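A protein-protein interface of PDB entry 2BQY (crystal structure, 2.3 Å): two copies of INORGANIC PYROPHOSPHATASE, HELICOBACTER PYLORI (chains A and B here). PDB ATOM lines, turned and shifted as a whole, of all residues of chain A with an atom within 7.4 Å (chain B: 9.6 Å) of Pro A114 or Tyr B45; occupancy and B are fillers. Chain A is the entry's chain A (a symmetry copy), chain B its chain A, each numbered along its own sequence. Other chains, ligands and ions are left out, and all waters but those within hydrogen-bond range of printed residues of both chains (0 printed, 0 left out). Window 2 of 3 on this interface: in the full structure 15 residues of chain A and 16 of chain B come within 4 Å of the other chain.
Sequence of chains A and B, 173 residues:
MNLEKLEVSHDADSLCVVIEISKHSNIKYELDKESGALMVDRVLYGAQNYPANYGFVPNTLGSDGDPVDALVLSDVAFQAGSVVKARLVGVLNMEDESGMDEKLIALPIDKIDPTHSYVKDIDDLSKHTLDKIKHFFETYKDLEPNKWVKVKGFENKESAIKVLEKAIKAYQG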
ATOM      1  N   ARG A  87      35.533   0.534  -1.225  1.00  0.00           N
ATOM      2  CA  ARG A  87      36.695   0.683  -0.362  1.00  0.00           C
ATOM      3  C   ARG A  87      37.902   1.010  -1.232  1.00  0.00           C
ATOM      4  O   ARG A  87      38.022   0.500  -2.341  1.00  0.00           O
ATOM      5  CB  ARG A  87      36.943  -0.613   0.419  1.00  0.00           C
ATOM      6  CG  ARG A  87      37.197  -1.844  -0.443  1.00  0.00           C
ATOM      7  CD  ARG A  87      37.247  -3.108   0.424  1.00  0.00           C
ATOM      8  NE  ARG A  87      37.527  -4.324  -0.332  1.00  0.00           N
ATOM      9  CZ  ARG A  87      38.720  -4.643  -0.817  1.00  0.00           C
ATOM     10  NH1 ARG A  87      38.877  -5.764  -1.494  1.00  0.00           N
ATOM     11  NH2 ARG A  87      39.762  -3.857  -0.617  1.00  0.00           N
ATOM     12  N   PRO A 108      34.096  -2.463  -4.719  1.00  0.00           N
ATOM     13  CA  PRO A 108      32.854  -2.470  -3.938  1.00  0.00           C
ATOM     14  C   PRO A 108      33.059  -3.219  -2.627  1.00  0.00           C
ATOM     15  O   PRO A 108      33.785  -4.207  -2.585  1.00  0.00           O
ATOM     16  CB  PRO A 108      31.858  -3.150  -4.876  1.00  0.00           C
ATOM     17  CG  PRO A 108      32.730  -4.085  -5.642  1.00  0.00           C
ATOM     18  CD  PRO A 108      33.940  -3.253  -5.953  1.00  0.00           C
ATOM     19  N   ILE A 109      32.437  -2.749  -1.551  1.00  0.00           N
ATOM     20  CA  ILE A 109      32.608  -3.406  -0.258  1.00  0.00           C
ATOM     21  C   ILE A 109      32.126  -4.852  -0.346  1.00  0.00           C
ATOM     22  O   ILE A 109      31.213  -5.156  -1.097  1.00  0.00           O
ATOM     23  CB  ILE A 109      31.836  -2.668   0.861  1.00  0.00           C
ATOM     24  CG1 ILE A 109      30.327  -2.710   0.582  1.00  0.00           C
ATOM     25  CG2 ILE A 109      32.318  -1.217   0.944  1.00  0.00           C
ATOM     26  CD1 ILE A 109      29.489  -2.199   1.723  1.00  0.00           C
ATOM     27  N   ASP A 110      32.739  -5.742   0.423  1.00  0.00           N
ATOM     28  CA  ASP A 110      32.389  -7.161   0.405  1.00  0.00           C
ATOM     29  C   ASP A 110      30.924  -7.543   0.626  1.00  0.00           C
ATOM     30  O   ASP A 110      30.442  -8.486   0.013  1.00  0.00           O
ATOM     31  CB  ASP A 110      33.260  -7.916   1.410  1.00  0.00           C
ATOM     32  CG  ASP A 110      34.715  -7.948   1.007  1.00  0.00           C
ATOM     33  OD1 ASP A 110      35.016  -7.665  -0.168  1.00  0.00           O
ATOM     34  OD2 ASP A 110      35.563  -8.275   1.861  1.00  0.00           O
ATOM     35  N   LYS A 111      30.203  -6.831   1.485  1.00  0.00           N
ATOM     36  CA  LYS A 111      28.800  -7.194   1.706  1.00  0.00           C
ATOM     37  C   LYS A 111      28.006  -6.978   0.404  1.00  0.00           C
ATOM     38  O   LYS A 111      26.836  -7.384   0.294  1.00  0.00           O
ATOM     39  CB  LYS A 111      28.169  -6.373   2.848  1.00  0.00           C
ATOM     40  CG  LYS A 111      27.480  -5.096   2.418  1.00  0.00           C
ATOM     41  CD  LYS A 111      26.667  -4.501   3.562  1.00  0.00           C
ATOM     42  CE  LYS A 111      25.501  -5.432   3.937  1.00  0.00           C
ATOM     43  NZ  LYS A 111      24.486  -4.716   4.801  1.00  0.00           N
ATOM     44  N   ILE A 112      28.642  -6.315  -0.564  1.00  0.00           N
ATOM     45  CA  ILE A 112      28.031  -6.051  -1.867  1.00  0.00           C
ATOM     46  C   ILE A 112      28.537  -7.061  -2.902  1.00  0.00           C
ATOM     47  O   ILE A 112      27.752  -7.766  -3.538  1.00  0.00           O
ATOM     48  CB  ILE A 112      28.357  -4.625  -2.359  1.00  0.00           C
ATOM     49  CG1 ILE A 112      27.641  -3.607  -1.480  1.00  0.00           C
ATOM     50  CG2 ILE A 112      27.931  -4.460  -3.800  1.00  0.00           C
ATOM     51  CD1 ILE A 112      27.848  -2.171  -1.912  1.00  0.00           C
ATOM     52  N   ASP A 113      29.856  -7.127  -3.051  1.00  0.00           N
ATOM     53  CA  ASP A 113      30.497  -8.027  -4.006  1.00  0.00           C
ATOM     54  C   ASP A 113      31.908  -8.369  -3.533  1.00  0.00           C
ATOM     55  O   ASP A 113      32.811  -7.538  -3.587  1.00  0.00           O
ATOM     56  CB  ASP A 113      30.532  -7.356  -5.384  1.00  0.00           C
ATOM     57  CG  ASP A 113      31.237  -8.193  -6.437  1.00  0.00           C
ATOM     58  OD1 ASP A 113      31.396  -9.418  -6.216  1.00  0.00           O
ATOM     59  OD2 ASP A 113      31.617  -7.607  -7.480  1.00  0.00           O
ATOM     60  N   PRO A 114      32.109  -9.614  -3.076  1.00  0.00           N
ATOM     61  CA  PRO A 114      33.400 -10.091  -2.575  1.00  0.00           C
ATOM     62  C   PRO A 114      34.320 -10.816  -3.554  1.00  0.00           C
ATOM     63  O   PRO A 114      35.202 -11.553  -3.131  1.00  0.00           O
ATOM     64  CB  PRO A 114      32.986 -10.992  -1.425  1.00  0.00           C
ATOM     65  CG  PRO A 114      31.779 -11.683  -2.009  1.00  0.00           C
ATOM     66  CD  PRO A 114      31.026 -10.543  -2.697  1.00  0.00           C
ATOM     67  N   THR A 115      34.144 -10.595  -4.850  1.00  0.00           N
ATOM     68  CA  THR A 115      34.974 -11.282  -5.835  1.00  0.00           C
ATOM     69  C   THR A 115      36.453 -10.967  -5.657  1.00  0.00           C
ATOM     70  O   THR A 115      37.311 -11.829  -5.828  1.00  0.00           O
ATOM     71  CB  THR A 115      34.586 -10.907  -7.262  1.00  0.00           C
ATOM     72  OG1 THR A 115      33.158 -10.923  -7.384  1.00  0.00           O
ATOM     73  CG2 THR A 115      35.195 -11.905  -8.253  1.00  0.00           C
ATOM     74  N   HIS A 116      36.752  -9.719  -5.305  1.00  0.00           N
ATOM     75  CA  HIS A 116      38.140  -9.294  -5.117  1.00  0.00           C
ATOM     76  C   HIS A 116      38.440  -8.881  -3.680  1.00  0.00           C
ATOM     77  O   HIS A 116      39.220  -7.962  -3.440  1.00  0.00           O
ATOM     78  CB  HIS A 116      38.472  -8.131  -6.066  1.00  0.00           C
ATOM     79  CG  HIS A 116      38.257  -8.455  -7.512  1.00  0.00           C
ATOM     80  ND1 HIS A 116      39.035  -9.364  -8.191  1.00  0.00           N
ATOM     81  CD2 HIS A 116      37.337  -8.009  -8.400  1.00  0.00           C
ATOM     82  CE1 HIS A 116      38.605  -9.463  -9.437  1.00  0.00           C
ATOM     83  NE2 HIS A 116      37.576  -8.653  -9.589  1.00  0.00           N
ATOM     84  N   SER A 117      37.818  -9.561  -2.722  1.00  0.00           N
ATOM     85  CA  SER A 117      38.036  -9.263  -1.310  1.00  0.00           C
ATOM     86  C   SER A 117      39.505  -9.482  -0.932  1.00  0.00           C
ATOM     87  O   SER A 117      39.996  -8.911   0.044  1.00  0.00           O
ATOM     88  CB  SER A 117      37.144 -10.154  -0.441  1.00  0.00           C
ATOM     89  OG  SER A 117      37.498 -11.513  -0.632  1.00  0.00           O
ATOM     90  N   TYR A 118      40.197 -10.306  -1.714  1.00  0.00           N
ATOM     91  CA  TYR A 118      41.601 -10.608  -1.469  1.00  0.00           C
ATOM     92  C   TYR A 118      42.501  -9.414  -1.783  1.00  0.00           C
ATOM     93  O   TYR A 118      43.648  -9.359  -1.320  1.00  0.00           O
ATOM     94  CB  TYR A 118      42.024 -11.821  -2.301  1.00  0.00           C
ATOM     95  CG  TYR A 118      41.915 -11.611  -3.799  1.00  0.00           C
ATOM     96  CD1 TYR A 118      42.985 -11.099  -4.523  1.00  0.00           C
ATOM     97  CD2 TYR A 118      40.730 -11.908  -4.487  1.00  0.00           C
ATOM     98  CE1 TYR A 118      42.883 -10.885  -5.894  1.00  0.00           C
ATOM     99  CE2 TYR A 118      40.615 -11.698  -5.851  1.00  0.00           C
ATOM    100  CZ  TYR A 118      41.696 -11.185  -6.552  1.00  0.00           C
ATOM    101  OH  TYR A 118      41.594 -10.965  -7.908  1.00  0.00           O
ATOM    102  N   ASN B  26      22.358  -9.820 -12.795  1.00  0.00           N
ATOM    103  CA  ASN B  26      22.894 -10.453 -11.598  1.00  0.00           C
ATOM    104  C   ASN B  26      23.221  -9.385 -10.551  1.00  0.00           C
ATOM    105  O   ASN B  26      23.804  -9.676  -9.504  1.00  0.00           O
ATOM    106  CB  ASN B  26      24.153 -11.260 -11.942  1.00  0.00           C
ATOM    107  CG  ASN B  26      25.316 -10.386 -12.369  1.00  0.00           C
ATOM    108  OD1 ASN B  26      25.150  -9.317 -12.934  1.00  0.00           O
ATOM    109  ND2 ASN B  26      26.501 -10.863 -12.113  1.00  0.00           N
ATOM    110  N   ILE B  27      22.874  -8.141 -10.857  1.00  0.00           N
ATOM    111  CA  ILE B  27      23.137  -7.038  -9.952  1.00  0.00           C
ATOM    112  C   ILE B  27      21.831  -6.610  -9.301  1.00  0.00           C
ATOM    113  O   ILE B  27      20.899  -6.175  -9.970  1.00  0.00           O
ATOM    114  CB  ILE B  27      23.740  -5.825 -10.698  1.00  0.00           C
ATOM    115  CG1 ILE B  27      25.059  -6.221 -11.365  1.00  0.00           C
ATOM    116  CG2 ILE B  27      23.930  -4.655  -9.730  1.00  0.00           C
ATOM    117  CD1 ILE B  27      25.597  -5.165 -12.306  1.00  0.00           C
ATOM    118  N   LYS B  28      21.772  -6.760  -7.985  1.00  0.00           N
ATOM    119  CA  LYS B  28      20.597  -6.384  -7.217  1.00  0.00           C
ATOM    120  C   LYS B  28      20.659  -4.940  -6.705  1.00  0.00           C
ATOM    121  O   LYS B  28      21.475  -4.611  -5.834  1.00  0.00           O
ATOM    122  CB  LYS B  28      20.428  -7.346  -6.035  1.00  0.00           C
ATOM    123  CG  LYS B  28      19.451  -6.868  -4.972  1.00  0.00           C
ATOM    124  CD  LYS B  28      19.157  -7.971  -3.959  1.00  0.00           C
ATOM    125  CE  LYS B  28      18.334  -7.446  -2.780  1.00  0.00           C
ATOM    126  NZ  LYS B  28      17.041  -6.846  -3.207  1.00  0.00           N
ATOM    127  N   ASP B  41      22.881  -2.829  -3.976  1.00  0.00           N
ATOM    128  CA  ASP B  41      22.788  -3.679  -2.790  1.00  0.00           C
ATOM    129  C   ASP B  41      23.757  -4.852  -2.837  1.00  0.00           C
ATOM    130  O   ASP B  41      24.398  -5.152  -1.830  1.00  0.00           O
ATOM    131  CB  ASP B  41      21.353  -4.177  -2.621  1.00  0.00           C
ATOM    132  CG  ASP B  41      21.044  -4.559  -1.189  1.00  0.00           C
ATOM    133  OD1 ASP B  41      21.225  -3.712  -0.290  1.00  0.00           O
ATOM    134  OD2 ASP B  41      20.632  -5.709  -0.950  1.00  0.00           O
ATOM    135  N   ARG B  42      23.853  -5.520  -3.983  1.00  0.00           N
ATOM    136  CA  ARG B  42      24.799  -6.631  -4.123  1.00  0.00           C
ATOM    137  C   ARG B  42      24.855  -7.268  -5.493  1.00  0.00           C
ATOM    138  O   ARG B  42      23.967  -7.067  -6.305  1.00  0.00           O
ATOM    139  CB  ARG B  42      24.499  -7.725  -3.113  1.00  0.00           C
ATOM    140  CG  ARG B  42      23.383  -8.640  -3.528  1.00  0.00           C
ATOM    141  CD  ARG B  42      23.165  -9.756  -2.509  1.00  0.00           C
ATOM    142  NE  ARG B  42      23.176  -9.254  -1.132  1.00  0.00           N
ATOM    143  CZ  ARG B  42      24.286  -9.099  -0.412  1.00  0.00           C
ATOM    144  NH1 ARG B  42      24.242  -8.621   0.837  1.00  0.00           N
ATOM    145  NH2 ARG B  42      25.451  -9.464  -0.943  1.00  0.00           N
ATOM    146  N   VAL B  43      25.910  -8.047  -5.721  1.00  0.00           N
ATOM    147  CA  VAL B  43      26.109  -8.772  -6.967  1.00  0.00           C
ATOM    148  C   VAL B  43      25.984 -10.232  -6.570  1.00  0.00           C
ATOM    149  O   VAL B  43      26.687 -10.684  -5.674  1.00  0.00           O
ATOM    150  CB  VAL B  43      27.522  -8.524  -7.565  1.00  0.00           C
ATOM    151  CG1 VAL B  43      27.660  -9.254  -8.873  1.00  0.00           C
ATOM    152  CG2 VAL B  43      27.761  -7.051  -7.764  1.00  0.00           C
ATOM    153  N   LEU B  44      25.088 -10.960  -7.230  1.00  0.00           N
ATOM    154  CA  LEU B  44      24.860 -12.367  -6.921  1.00  0.00           C
ATOM    155  C   LEU B  44      26.154 -13.170  -6.839  1.00  0.00           C
ATOM    156  O   LEU B  44      26.966 -13.148  -7.764  1.00  0.00           O
ATOM    157  CB  LEU B  44      23.926 -12.988  -7.960  1.00  0.00           C
ATOM    158  CG  LEU B  44      22.519 -12.387  -7.996  1.00  0.00           C
ATOM    159  CD1 LEU B  44      21.683 -13.141  -8.999  1.00  0.00           C
ATOM    160  CD2 LEU B  44      21.868 -12.456  -6.616  1.00  0.00           C
ATOM    161  N   TYR B  45      26.332 -13.851  -5.709  1.00  0.00           N
ATOM    162  CA  TYR B  45      27.507 -14.676  -5.442  1.00  0.00           C
ATOM    163  C   TYR B  45      27.689 -15.824  -6.425  1.00  0.00           C
ATOM    164  O   TYR B  45      28.816 -16.160  -6.776  1.00  0.00           O
ATOM    165  CB  TYR B  45      27.427 -15.242  -4.021  1.00  0.00           C
ATOM    166  CG  TYR B  45      27.803 -14.253  -2.922  1.00  0.00           C
ATOM    167  CD1 TYR B  45      27.459 -12.904  -3.016  1.00  0.00           C
ATOM    168  CD2 TYR B  45      28.463 -14.682  -1.769  1.00  0.00           C
ATOM    169  CE1 TYR B  45      27.758 -12.016  -2.000  1.00  0.00           C
ATOM    170  CE2 TYR B  45      28.767 -13.799  -0.739  1.00  0.00           C
ATOM    171  CZ  TYR B  45      28.414 -12.468  -0.860  1.00  0.00           C
ATOM    172  OH  TYR B  45      28.731 -11.578   0.138  1.00  0.00           O
ATOM    173  N   GLY B  46      26.585 -16.407  -6.876  1.00  0.00           N
ATOM    174  CA  GLY B  46      26.667 -17.525  -7.800  1.00  0.00           C
ATOM    175  C   GLY B  46      26.452 -17.161  -9.250  1.00  0.00           C
ATOM    176  O   GLY B  46      26.148 -16.007  -9.557  1.00  0.00           O
ATOM    177  N   ALA B  47      26.604 -18.153 -10.129  1.00  0.00           N
ATOM    178  CA  ALA B  47      26.444 -17.955 -11.566  1.00  0.00           C
ATOM    179  C   ALA B  47      24.960 -17.964 -11.877  1.00  0.00           C
ATOM    180  O   ALA B  47      24.459 -18.850 -12.546  1.00  0.00           O
ATOM    181  CB  ALA B  47      27.154 -19.054 -12.326  1.00  0.00           C
ATOM    182  N   GLN B  48      24.261 -16.957 -11.367  1.00  0.00           N
ATOM    183  CA  GLN B  48      22.819 -16.832 -11.551  1.00  0.00           C
ATOM    184  C   GLN B  48      22.422 -15.456 -12.053  1.00  0.00           C
ATOM    185  O   GLN B  48      23.247 -14.569 -12.178  1.00  0.00           O
ATOM    186  CB  GLN B  48      22.091 -17.108 -10.232  1.00  0.00           C
ATOM    187  CG  GLN B  48      22.228 -18.531  -9.729  1.00  0.00           C
ATOM    188  CD  GLN B  48      21.759 -18.694  -8.297  1.00  0.00           C
ATOM    189  OE1 GLN B  48      22.481 -18.367  -7.365  1.00  0.00           O
ATOM    190  NE2 GLN B  48      20.542 -19.188  -8.117  1.00  0.00           N
ATOM    191  N   ASN B  49      21.136 -15.302 -12.343  1.00  0.00           N
ATOM    192  CA  ASN B  49      20.573 -14.049 -12.837  1.00  0.00           C
ATOM    193  C   ASN B  49      19.072 -14.098 -12.607  1.00  0.00           C
ATOM    194  O   ASN B  49      18.454 -15.142 -12.777  1.00  0.00           O
ATOM    195  CB  ASN B  49      20.863 -13.864 -14.335  1.00  0.00           C
ATOM    196  CG  ASN B  49      20.566 -15.109 -15.153  1.00  0.00           C
ATOM    197  OD1 ASN B  49      21.373 -16.055 -15.215  1.00  0.00           O
ATOM    198  ND2 ASN B  49      19.389 -15.128 -15.771  1.00  0.00           N
ATOM    199  N   TYR B  50      18.490 -12.971 -12.217  1.00  0.00           N
ATOM    200  CA  TYR B  50      17.060 -12.920 -11.939  1.00  0.00           C
ATOM    201  C   TYR B  50      16.189 -13.418 -13.069  1.00  0.00           C
ATOM    202  O   TYR B  50      16.365 -13.025 -14.208  1.00  0.00           O
ATOM    203  CB  TYR B  50      16.646 -11.508 -11.532  1.00  0.00           C
ATOM    204  CG  TYR B  50      17.074 -11.160 -10.120  1.00  0.00           C
ATOM    205  CD1 TYR B  50      18.422 -10.929  -9.814  1.00  0.00           C
ATOM    206  CD2 TYR B  50      16.140 -11.107  -9.085  1.00  0.00           C
ATOM    207  CE1 TYR B  50      18.835 -10.655  -8.520  1.00  0.00           C
ATOM    208  CE2 TYR B  50      16.541 -10.836  -7.780  1.00  0.00           C
ATOM    209  CZ  TYR B  50      17.894 -10.613  -7.507  1.00  0.00           C
ATOM    210  OH  TYR B  50      18.297 -10.362  -6.220  1.00  0.00           O
ATOM    211  N   PHE B 136      15.409 -20.429  -8.286  1.00  0.00           N
ATOM    212  CA  PHE B 136      16.297 -19.283  -8.180  1.00  0.00           C
ATOM    213  C   PHE B 136      16.363 -18.791  -6.732  1.00  0.00           C
ATOM    214  O   PHE B 136      17.451 -18.626  -6.168  1.00  0.00           O
ATOM    215  CB  PHE B 136      15.801 -18.148  -9.094  1.00  0.00           C
ATOM    216  CG  PHE B 136      16.560 -16.862  -8.930  1.00  0.00           C
ATOM    217  CD1 PHE B 136      17.804 -16.692  -9.522  1.00  0.00           C
ATOM    218  CD2 PHE B 136      16.042 -15.828  -8.153  1.00  0.00           C
ATOM    219  CE1 PHE B 136      18.537 -15.490  -9.336  1.00  0.00           C
ATOM    220  CE2 PHE B 136      16.764 -14.621  -7.957  1.00  0.00           C
ATOM    221  CZ  PHE B 136      18.013 -14.459  -8.551  1.00  0.00           C
ATOM    222  N   THR B 139      17.992 -20.975  -4.064  1.00  0.00           N
ATOM    223  CA  THR B 139      19.443 -21.159  -4.128  1.00  0.00           C
ATOM    224  C   THR B 139      20.308 -19.910  -4.320  1.00  0.00           C
ATOM    225  O   THR B 139      21.508 -19.943  -4.072  1.00  0.00           O
ATOM    226  CB  THR B 139      19.807 -22.149  -5.265  1.00  0.00           C
ATOM    227  OG1 THR B 139      19.372 -21.611  -6.519  1.00  0.00           O
ATOM    228  CG2 THR B 139      19.144 -23.502  -5.050  1.00  0.00           C
ATOM    229  N   TYR B 140      19.707 -18.807  -4.744  1.00  0.00           N
ATOM    230  CA  TYR B 140      20.472 -17.591  -5.000  1.00  0.00           C
ATOM    231  C   TYR B 140      21.178 -17.003  -3.776  1.00  0.00           C
ATOM    232  O   TYR B 140      21.942 -16.037  -3.904  1.00  0.00           O
ATOM    233  CB  TYR B 140      19.594 -16.520  -5.684  1.00  0.00           C
ATOM    234  CG  TYR B 140      18.746 -15.669  -4.757  1.00  0.00           C
ATOM    235  CD1 TYR B 140      17.923 -16.249  -3.788  1.00  0.00           C
ATOM    236  CD2 TYR B 140      18.756 -14.281  -4.868  1.00  0.00           C
ATOM    237  CE1 TYR B 140      17.132 -15.462  -2.949  1.00  0.00           C
ATOM    238  CE2 TYR B 140      17.973 -13.481  -4.043  1.00  0.00           C
ATOM    239  CZ  TYR B 140      17.158 -14.071  -3.083  1.00  0.00           C
ATOM    240  OH  TYR B 140      16.365 -13.273  -2.276  1.00  0.00           O
ATOM    241  N   LYS B 141      20.930 -17.582  -2.601  1.00  0.00           N
ATOM    242  CA  LYS B 141      21.585 -17.101  -1.387  1.00  0.00           C
ATOM    243  C   LYS B 141      22.387 -18.189  -0.692  1.00  0.00           C
ATOM    244  O   LYS B 141      22.784 -18.030   0.444  1.00  0.00           O
ATOM    245  CB  LYS B 141      20.567 -16.494  -0.411  1.00  0.00           C
ATOM    246  CG  LYS B 141      20.183 -15.052  -0.738  1.00  0.00           C
ATOM    247  CD  LYS B 141      19.673 -14.296   0.475  1.00  0.00           C
ATOM    248  CE  LYS B 141      18.204 -14.503   0.721  1.00  0.00           C
ATOM    249  NZ  LYS B 141      17.740 -13.867   2.020  1.00  0.00           N
ATOM    250  N   ASP B 142      22.644 -19.281  -1.398  1.00  0.00           N
ATOM    251  CA  ASP B 142      23.398 -20.403  -0.845  1.00  0.00           C
ATOM    252  C   ASP B 142      24.808 -20.021  -0.395  1.00  0.00           C
ATOM    253  O   ASP B 142      25.241 -20.410   0.697  1.00  0.00           O
ATOM    254  CB  ASP B 142      23.511 -21.547  -1.870  1.00  0.00           C
ATOM    255  CG  ASP B 142      22.179 -22.219  -2.156  1.00  0.00           C
ATOM    256  OD1 ASP B 142      21.189 -21.912  -1.470  1.00  0.00           O
ATOM    257  OD2 ASP B 142      22.119 -23.075  -3.064  1.00  0.00           O
ATOM    258  N   LEU B 143      25.510 -19.256  -1.223  1.00  0.00           N
ATOM    259  CA  LEU B 143      26.876 -18.874  -0.913  1.00  0.00           C
ATOM    260  C   LEU B 143      27.033 -17.668   0.001  1.00  0.00           C
ATOM    261  O   LEU B 143      28.148 -17.324   0.387  1.00  0.00           O
ATOM    262  CB  LEU B 143      27.641 -18.650  -2.221  1.00  0.00           C
ATOM    263  CG  LEU B 143      27.704 -19.857  -3.168  1.00  0.00           C
ATOM    264  CD1 LEU B 143      28.006 -19.375  -4.564  1.00  0.00           C
ATOM    265  CD2 LEU B 143      28.729 -20.875  -2.685  1.00  0.00           C
ATOM    266  N   GLU B 144      25.916 -17.038   0.357  1.00  0.00           N
ATOM    267  CA  GLU B 144      25.970 -15.870   1.228  1.00  0.00           C
ATOM    268  C   GLU B 144      25.895 -16.278   2.692  1.00  0.00           C
ATOM    269  O   GLU B 144      24.861 -16.734   3.159  1.00  0.00           O
ATOM    270  CB  GLU B 144      24.827 -14.905   0.896  1.00  0.00           C
ATOM    271  CG  GLU B 144      24.998 -14.183  -0.426  1.00  0.00           C
ATOM    272  CD  GLU B 144      23.941 -13.135  -0.654  1.00  0.00           C
ATOM    273  OE1 GLU B 144      23.702 -12.349   0.285  1.00  0.00           O
ATOM    274  OE2 GLU B 144      23.368 -13.078  -1.766  1.00  0.00           O
ATOM    275  N   PRO B 145      27.004 -16.132   3.435  1.00  0.00           N
ATOM    276  CA  PRO B 145      27.090 -16.480   4.857  1.00  0.00           C
ATOM    277  C   PRO B 145      25.892 -16.048   5.695  1.00  0.00           C
ATOM    278  O   PRO B 145      25.383 -14.913   5.553  1.00  0.00           O
ATOM    279  CB  PRO B 145      28.366 -15.785   5.309  1.00  0.00           C
ATOM    280  CG  PRO B 145      29.229 -15.917   4.118  1.00  0.00           C
ATOM    281  CD  PRO B 145      28.276 -15.536   2.982  1.00  0.00           C
ATOM    282  N   ASN B 146      25.450 -16.963   6.560  1.00  0.00           N
ATOM    283  CA  ASN B 146      24.328 -16.706   7.467  1.00  0.00           C
ATOM    284  C   ASN B 146      23.045 -16.228   6.758  1.00  0.00           C
ATOM    285  O   ASN B 146      22.228 -15.500   7.336  1.00  0.00           O
ATOM    286  CB  ASN B 146      24.736 -15.669   8.524  1.00  0.00           C
ATOM    287  CG  ASN B 146      26.051 -16.004   9.179  1.00  0.00           C
ATOM    288  OD1 ASN B 146      27.046 -15.280   9.010  1.00  0.00           O
ATOM    289  ND2 ASN B 146      26.083 -17.126   9.913  1.00  0.00           N
ATOM    290  N   LYS B 147      22.880 -16.627   5.503  1.00  0.00           N
ATOM    291  CA  LYS B 147      21.691 -16.261   4.739  1.00  0.00           C
ATOM    292  C   LYS B 147      21.139 -17.527   4.093  1.00  0.00           C
ATOM    293  O   LYS B 147      21.918 -18.431   3.700  1.00  0.00           O
ATOM    294  CB  LYS B 147      22.024 -15.230   3.654  1.00  0.00           C
ATOM    295  CG  LYS B 147      22.369 -13.853   4.188  1.00  0.00           C
ATOM    296  CD  LYS B 147      22.637 -12.883   3.053  1.00  0.00           C
ATOM    297  CE  LYS B 147      23.095 -11.521   3.574  1.00  0.00           C
ATOM    298  NZ  LYS B 147      22.131 -11.015   4.623  1.00  0.00           N
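The guanidinium group of Arg B42 sits at hydrogen-bond distance from the backbone carbonyl oxygen of Lys A111, at 2.8 Å. O of Ile A112 is in hydrogen-bond range of N of Val B43.
The backbone NH (N) of Asp B41 lies within hydrogen-bond range of the backbone carbonyl oxygen (O) of Lys B28 (2.9 Å). The backbone carbonyl oxygen (O) of Arg B42 is in hydrogen-bond range of the backbone NH (N) of Lys B28 (2.8 Å). The side-chain carboxylate (OE1) of Glu B144 lies within salt-bridge range of the guanidinium group (NE) of Arg B42. The side-chain carboxylate of Asp A113 is in hydrogen-bond range of the side-chain hydroxyl of Thr A115 (2.6 Å). The backbone carbonyl oxygen (O) of Pro A114 lies within hydrogen-bond range of the side-chain hydroxyl (OG) of Ser A117, at 3.4 Å.
Among the printed residues, merely in contact across the chains: Ile A112 with Arg B42, Asp A110 with Tyr B45, Ile A112 with Asp B41, Pro A114 with Tyr B45, Asp A113 with Val B43 and Lys A111 with Asp B41.
Pro A108 touches none of the printed residues of chain B. Asp A110 touches one residue of chain B. Of the printed residues of chain B, Lys A111 touches Asp B41 (3.9 Å) and Arg B42 (2.8 Å). Asp A113 touches one residue of chain B. Of the printed residues of chain B, Pro A114 touches Tyr B45 (3.6 Å). No residue of chain B comes within 4 Å of Thr A115. Of the printed residues of chain A, Asp B41 touches Lys A111 (3.9 Å) and Ile A112 (3.6 Å). Of the printed residues of chain A, Arg B42 touches Lys A111 (2.8 Å) and Ile A112 (3.2 Å). Tyr B45 touches just these residues of chain A: Asp A110 (3.5 Å) and Pro A114 (3.6 Å). Gly B46 touches none of the printed residues of chain A. The nearest residue of chain B that does not touch Pro A114 is Val B43 (5.3 Å). The nearest residue of chain A that does not touch Tyr B45 is Ile A112 (4.5 Å).
Printed residues of chain A that touch a printed residue of chain B: Asp A110, Lys A111, Ile A112, Asp A113 and Pro A114. Hydrophobic or aromatic side chains of chain A that line the printed part of chain B: Ile A112 and Pro A114. Along chain B the printed residues that touch a printed residue of chain A span positions 41 to 45. Among the printed residues, 8 pairs touch across the chains. Among the printed residues, no Asp or Glu carboxylate lies within 4 Å of a Lys or Arg side-chain nitrogen of the other chain.
No position is printed for both chains. Of the 8 pairs that touch across the chains among the printed residues, none has its exchanged pair printed and touching as well.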
